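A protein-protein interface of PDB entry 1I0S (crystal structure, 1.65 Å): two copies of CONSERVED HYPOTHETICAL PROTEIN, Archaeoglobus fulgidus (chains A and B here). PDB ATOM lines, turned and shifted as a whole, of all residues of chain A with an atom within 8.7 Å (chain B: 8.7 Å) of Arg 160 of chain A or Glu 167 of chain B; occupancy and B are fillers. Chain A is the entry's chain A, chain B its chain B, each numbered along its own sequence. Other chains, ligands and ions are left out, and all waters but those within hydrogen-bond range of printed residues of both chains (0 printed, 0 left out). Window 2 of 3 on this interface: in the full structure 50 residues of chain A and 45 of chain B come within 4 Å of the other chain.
NH1 of Arg 160 of chain A lies within salt-bridge range of OE1 of Glu 167 of chain B. N of Arg 160 of chain A sits at hydrogen-bond distance from O of Tyr 165 of chain B. The backbone carbonyl oxygen (O) of Thr 158 of chain A lies within hydrogen-bond range of the backbone NH (N) of Glu 167 of chain B, at 2.7 Å.
The backbone carbonyl oxygen of Glu 143 of chain A lies within hydrogen-bond range of the backbone NH of Leu 69 of chain A. The backbone carbonyl oxygen (O) of Leu 152 of chain A sits at hydrogen-bond distance from the backbone NH (N) of Lys 157 of chain A (3.1 Å).
CD2 of Leu 69 of chain A touches CG1 of Val 164 of chain B, 3.8 Å away. CD1 of Leu 152 of chain A touches CD1 of Phe 166 of chain B, 3.6 Å away. Phe 166 of chain B touches Lys 157 of chain A. CA of Lys 157 of chain A touches O of Glu 167 of chain B (3.5 Å). Thr 158 of chain A touches Tyr 165 of chain B (O to O, 3.9 Å). O of Thr 158 of chain A touches CA of Phe 166 of chain B, at 3.4 Å. Tyr 165 of chain B touches Pro 159 of chain A. Pro 159 of chain A touches Phe 166 of chain B.
Glu 70 of chain A touches none of the printed residues of chain B. Glu 143 of chain A touches none of the printed residues of chain B. Of the printed residues of chain B, Pro 159 of chain A touches Tyr 165 (3.5 Å) and Phe 166 (3.7 Å). Arg 160 of chain A touches just these residues of chain B: Tyr 165 (2.7 Å) and Glu 167 (3.5 Å). No residue of chain B comes within 4 Å of Thr 161 of chain A. Of the printed residues of chain A, Val 164 of chain B touches Leu 69. Glu 167 of chain B touches just these residues of chain A: Lys 157 (3.5 Å), Thr 158 (2.7 Å) and Arg 160 (3.5 Å). The nearest residue of chain B that does not touch Arg 160 of chain A is Val 164 of chain B (4.6 Å).
Of the 7 printed residues of chain B, 4 touch a printed residue of chain A. Hydrophobic or aromatic side chains of chain B that line the printed part of chain A: Val 164, Tyr 165 and Phe 166. Among the printed residues, 11 pairs touch across the chains. Among the printed residues, Asp or Glu carboxylates within 4 Å of a Lys or Arg side-chain nitrogen of the other chain: Arg 160 of chain A with Glu 167 of chain B.
No position is printed for both chains. Of the 11 pairs that touch across the chains among the printed residues, none has its exchanged pair printed and touching as well.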
ATOM      1  N   LEU A  69     -26.891  -5.126   1.422  1.00  0.00           N
ATOM      2  CA  LEU A  69     -27.140  -4.093   2.422  1.00  0.00           C
ATOM      3  C   LEU A  69     -28.106  -4.543   3.523  1.00  0.00           C
ATOM      4  O   LEU A  69     -27.892  -4.267   4.701  1.00  0.00           O
ATOM      5  CB  LEU A  69     -27.697  -2.845   1.724  1.00  0.00           C
ATOM      6  CG  LEU A  69     -28.153  -1.665   2.603  1.00  0.00           C
ATOM      7  CD1 LEU A  69     -26.982  -1.071   3.349  1.00  0.00           C
ATOM      8  CD2 LEU A  69     -28.792  -0.594   1.718  1.00  0.00           C
ATOM      9  N   GLU A  70     -29.169  -5.241   3.136  1.00  0.00           N
ATOM     10  CA  GLU A  70     -30.165  -5.672   4.111  1.00  0.00           C
ATOM     11  C   GLU A  70     -29.884  -6.994   4.817  1.00  0.00           C
ATOM     12  O   GLU A  70     -30.801  -7.628   5.333  1.00  0.00           O
ATOM     13  CB  GLU A  70     -31.548  -5.697   3.435  1.00  0.00           C
ATOM     14  CG  GLU A  70     -31.800  -4.383   2.710  1.00  0.00           C
ATOM     15  CD  GLU A  70     -33.138  -4.288   2.013  1.00  0.00           C
ATOM     16  OE1 GLU A  70     -33.566  -5.269   1.370  1.00  0.00           O
ATOM     17  OE2 GLU A  70     -33.753  -3.208   2.095  1.00  0.00           O
ATOM     18  N   GLU A 143     -28.038  -3.387  -3.204  1.00  0.00           N
ATOM     19  CA  GLU A 143     -26.851  -2.623  -2.844  1.00  0.00           C
ATOM     20  C   GLU A 143     -26.017  -3.543  -1.966  1.00  0.00           C
ATOM     21  O   GLU A 143     -26.553  -4.460  -1.333  1.00  0.00           O
ATOM     22  CB  GLU A 143     -27.205  -1.364  -2.039  1.00  0.00           C
ATOM     23  CG  GLU A 143     -27.978  -0.320  -2.812  1.00  0.00           C
ATOM     24  CD  GLU A 143     -27.206   0.171  -4.016  1.00  0.00           C
ATOM     25  OE1 GLU A 143     -26.119   0.755  -3.822  1.00  0.00           O
ATOM     26  OE2 GLU A 143     -27.685  -0.038  -5.154  1.00  0.00           O
ATOM     27  N   LEU A 152     -22.413   1.173  11.527  1.00  0.00           N
ATOM     28  CA  LEU A 152     -23.571   2.002  11.838  1.00  0.00           C
ATOM     29  C   LEU A 152     -24.658   1.073  12.400  1.00  0.00           C
ATOM     30  O   LEU A 152     -25.418   1.476  13.278  1.00  0.00           O
ATOM     31  CB  LEU A 152     -24.093   2.722  10.594  1.00  0.00           C
ATOM     32  CG  LEU A 152     -23.187   3.766   9.948  1.00  0.00           C
ATOM     33  CD1 LEU A 152     -23.916   4.312   8.746  1.00  0.00           C
ATOM     34  CD2 LEU A 152     -22.840   4.892  10.924  1.00  0.00           C
ATOM     35  N   MET A 153     -24.724  -0.163  11.896  1.00  0.00           N
ATOM     36  CA  MET A 153     -25.699  -1.153  12.377  1.00  0.00           C
ATOM     37  C   MET A 153     -25.353  -1.526  13.813  1.00  0.00           C
ATOM     38  O   MET A 153     -26.235  -1.773  14.644  1.00  0.00           O
ATOM     39  CB  MET A 153     -25.663  -2.431  11.520  1.00  0.00           C
ATOM     40  CG  MET A 153     -26.180  -2.274  10.093  1.00  0.00           C
ATOM     41  SD  MET A 153     -25.756  -3.723   9.071  1.00  0.00           S
ATOM     42  CE  MET A 153     -26.783  -4.993   9.790  1.00  0.00           C
ATOM     43  N   LYS A 155     -24.232   0.366  15.962  1.00  0.00           N
ATOM     44  CA  LYS A 155     -24.659   1.447  16.824  1.00  0.00           C
ATOM     45  C   LYS A 155     -26.183   1.480  16.937  1.00  0.00           C
ATOM     46  O   LYS A 155     -26.763   2.473  17.399  1.00  0.00           O
ATOM     47  CB  LYS A 155     -24.139   2.802  16.294  1.00  0.00           C
ATOM     48  CG  LYS A 155     -22.622   2.904  16.260  1.00  0.00           C
ATOM     49  CD  LYS A 155     -22.181   4.328  15.999  1.00  0.00           C
ATOM     50  CE  LYS A 155     -20.671   4.411  15.834  1.00  0.00           C
ATOM     51  NZ  LYS A 155     -19.986   3.204  16.372  1.00  0.00           N
ATOM     52  N   GLY A 156     -26.861   0.505  16.381  1.00  0.00           N
ATOM     53  CA  GLY A 156     -28.311   0.488  16.423  1.00  0.00           C
ATOM     54  C   GLY A 156     -29.053   1.042  15.223  1.00  0.00           C
ATOM     55  O   GLY A 156     -30.280   1.057  15.223  1.00  0.00           O
ATOM     56  N   LYS A 157     -28.334   1.501  14.204  1.00  0.00           N
ATOM     57  CA  LYS A 157     -28.988   2.031  13.013  1.00  0.00           C
ATOM     58  C   LYS A 157     -29.382   0.899  12.070  1.00  0.00           C
ATOM     59  O   LYS A 157     -28.788  -0.176  12.092  1.00  0.00           O
ATOM     60  CB  LYS A 157     -28.069   3.003  12.276  1.00  0.00           C
ATOM     61  CG  LYS A 157     -27.797   4.300  13.008  1.00  0.00           C
ATOM     62  CD  LYS A 157     -27.088   5.269  12.080  1.00  0.00           C
ATOM     63  CE  LYS A 157     -26.964   6.650  12.692  1.00  0.00           C
ATOM     64  NZ  LYS A 157     -26.303   7.600  11.745  1.00  0.00           N
ATOM     65  N   THR A 158     -30.381   1.153  11.232  1.00  0.00           N
ATOM     66  CA  THR A 158     -30.851   0.151  10.290  1.00  0.00           C
ATOM     67  C   THR A 158     -31.027   0.777   8.902  1.00  0.00           C
ATOM     68  O   THR A 158     -31.502   1.903   8.775  1.00  0.00           O
ATOM     69  CB  THR A 158     -32.187  -0.455  10.768  1.00  0.00           C
ATOM     70  OG1 THR A 158     -32.466  -1.644  10.022  1.00  0.00           O
ATOM     71  CG2 THR A 158     -33.322   0.534  10.584  1.00  0.00           C
ATOM     72  N   PRO A 159     -30.634   0.052   7.843  1.00  0.00           N
ATOM     73  CA  PRO A 159     -30.734   0.519   6.456  1.00  0.00           C
ATOM     74  C   PRO A 159     -32.152   0.746   5.942  1.00  0.00           C
ATOM     75  O   PRO A 159     -33.063  -0.035   6.217  1.00  0.00           O
ATOM     76  CB  PRO A 159     -30.031  -0.587   5.662  1.00  0.00           C
ATOM     77  CG  PRO A 159     -29.107  -1.206   6.663  1.00  0.00           C
ATOM     78  CD  PRO A 159     -29.959  -1.256   7.896  1.00  0.00           C
ATOM     79  N   ARG A 160     -32.324   1.821   5.185  1.00  0.00           N
ATOM     80  CA  ARG A 160     -33.610   2.149   4.587  1.00  0.00           C
ATOM     81  C   ARG A 160     -33.305   2.512   3.140  1.00  0.00           C
ATOM     82  O   ARG A 160     -32.800   3.598   2.856  1.00  0.00           O
ATOM     83  CB  ARG A 160     -34.265   3.331   5.306  1.00  0.00           C
ATOM     84  CG  ARG A 160     -35.662   3.677   4.795  1.00  0.00           C
ATOM     85  CD  ARG A 160     -36.257   4.841   5.580  1.00  0.00           C
ATOM     86  NE  ARG A 160     -37.580   5.247   5.102  1.00  0.00           N
ATOM     87  CZ  ARG A 160     -38.667   4.480   5.147  1.00  0.00           C
ATOM     88  NH1 ARG A 160     -38.595   3.254   5.648  1.00  0.00           N
ATOM     89  NH2 ARG A 160     -39.828   4.943   4.700  1.00  0.00           N
ATOM     90  N   THR A 161     -33.588   1.574   2.244  1.00  0.00           N
ATOM     91  CA  THR A 161     -33.356   1.732   0.811  1.00  0.00           C
ATOM     92  C   THR A 161     -33.524   3.163   0.285  1.00  0.00           C
ATOM     93  O   THR A 161     -34.569   3.452  -0.335  1.00  0.00           O
ATOM     94  CB  THR A 161     -34.280   0.788   0.018  1.00  0.00           C
ATOM     95  OG1 THR A 161     -35.637   0.984   0.437  1.00  0.00           O
ATOM     96  CG2 THR A 161     -33.887  -0.662   0.263  1.00  0.00           C
ATOM     97  N   ALA B 162     -24.948   8.599  -0.463  1.00  0.00           N
ATOM     98  CA  ALA B 162     -26.031   9.570  -0.429  1.00  0.00           C
ATOM     99  C   ALA B 162     -27.355   8.946  -0.862  1.00  0.00           C
ATOM    100  O   ALA B 162     -28.412   9.545  -0.682  1.00  0.00           O
ATOM    101  CB  ALA B 162     -25.694  10.751  -1.325  1.00  0.00           C
ATOM    102  N   THR B 163     -27.295   7.747  -1.435  1.00  0.00           N
ATOM    103  CA  THR B 163     -28.506   7.062  -1.886  1.00  0.00           C
ATOM    104  C   THR B 163     -28.977   6.050  -0.843  1.00  0.00           C
ATOM    105  O   THR B 163     -30.112   5.574  -0.888  1.00  0.00           O
ATOM    106  CB  THR B 163     -28.277   6.333  -3.227  1.00  0.00           C
ATOM    107  OG1 THR B 163     -27.279   5.320  -3.064  1.00  0.00           O
ATOM    108  CG2 THR B 163     -27.820   7.320  -4.291  1.00  0.00           C
ATOM    109  N   VAL B 164     -28.090   5.721   0.090  1.00  0.00           N
ATOM    110  CA  VAL B 164     -28.416   4.792   1.162  1.00  0.00           C
ATOM    111  C   VAL B 164     -28.701   5.624   2.409  1.00  0.00           C
ATOM    112  O   VAL B 164     -27.997   6.594   2.694  1.00  0.00           O
ATOM    113  CB  VAL B 164     -27.251   3.824   1.448  1.00  0.00           C
ATOM    114  CG1 VAL B 164     -27.602   2.916   2.612  1.00  0.00           C
ATOM    115  CG2 VAL B 164     -26.954   2.997   0.208  1.00  0.00           C
ATOM    116  N   TYR B 165     -29.735   5.241   3.147  1.00  0.00           N
ATOM    117  CA  TYR B 165     -30.128   5.967   4.347  1.00  0.00           C
ATOM    118  C   TYR B 165     -30.222   5.051   5.564  1.00  0.00           C
ATOM    119  O   TYR B 165     -30.754   3.945   5.478  1.00  0.00           O
ATOM    120  CB  TYR B 165     -31.476   6.650   4.085  1.00  0.00           C
ATOM    121  CG  TYR B 165     -32.137   7.275   5.291  1.00  0.00           C
ATOM    122  CD1 TYR B 165     -31.459   8.194   6.090  1.00  0.00           C
ATOM    123  CD2 TYR B 165     -33.459   6.964   5.615  1.00  0.00           C
ATOM    124  CE1 TYR B 165     -32.084   8.790   7.184  1.00  0.00           C
ATOM    125  CE2 TYR B 165     -34.091   7.551   6.702  1.00  0.00           C
ATOM    126  CZ  TYR B 165     -33.400   8.463   7.482  1.00  0.00           C
ATOM    127  OH  TYR B 165     -34.028   9.045   8.558  1.00  0.00           O
ATOM    128  N   PHE B 166     -29.692   5.510   6.694  1.00  0.00           N
ATOM    129  CA  PHE B 166     -29.739   4.727   7.922  1.00  0.00           C
ATOM    130  C   PHE B 166     -30.701   5.340   8.926  1.00  0.00           C
ATOM    131  O   PHE B 166     -30.624   6.526   9.242  1.00  0.00           O
ATOM    132  CB  PHE B 166     -28.346   4.591   8.537  1.00  0.00           C
ATOM    133  CG  PHE B 166     -27.463   3.627   7.804  1.00  0.00           C
ATOM    134  CD1 PHE B 166     -26.791   4.016   6.650  1.00  0.00           C
ATOM    135  CD2 PHE B 166     -27.345   2.311   8.238  1.00  0.00           C
ATOM    136  CE1 PHE B 166     -26.014   3.106   5.938  1.00  0.00           C
ATOM    137  CE2 PHE B 166     -26.572   1.394   7.533  1.00  0.00           C
ATOM    138  CZ  PHE B 166     -25.906   1.792   6.379  1.00  0.00           C
ATOM    139  N   GLU B 167     -31.605   4.504   9.422  1.00  0.00           N
ATOM    140  CA  GLU B 167     -32.627   4.914  10.372  1.00  0.00           C
ATOM    141  C   GLU B 167     -32.236   4.592  11.811  1.00  0.00           C
ATOM    142  O   GLU B 167     -32.065   3.428  12.177  1.00  0.00           O
ATOM    143  CB  GLU B 167     -33.936   4.210  10.013  1.00  0.00           C
ATOM    144  CG  GLU B 167     -35.155   4.650  10.790  1.00  0.00           C
ATOM    145  CD  GLU B 167     -36.417   4.012  10.248  1.00  0.00           C
ATOM    146  OE1 GLU B 167     -36.672   4.149   9.032  1.00  0.00           O
ATOM    147  OE2 GLU B 167     -37.152   3.371  11.030  1.00  0.00           O
ATOM    148  N   SER B 168     -32.096   5.636  12.623  1.00  0.00           N
ATOM    149  CA  SER B 168     -31.729   5.477  14.025  1.00  0.00           C
ATOM    150  C   SER B 168     -32.934   5.039  14.851  1.00  0.00           C
ATOM    151  O   SER B 168     -33.999   4.780  14.250  1.00  0.00           O
ATOM    152  CB  SER B 168     -31.172   6.793  14.580  1.00  0.00           C
ATOM    153  OG  SER B 168     -32.106   7.848  14.437  1.00  0.00           O
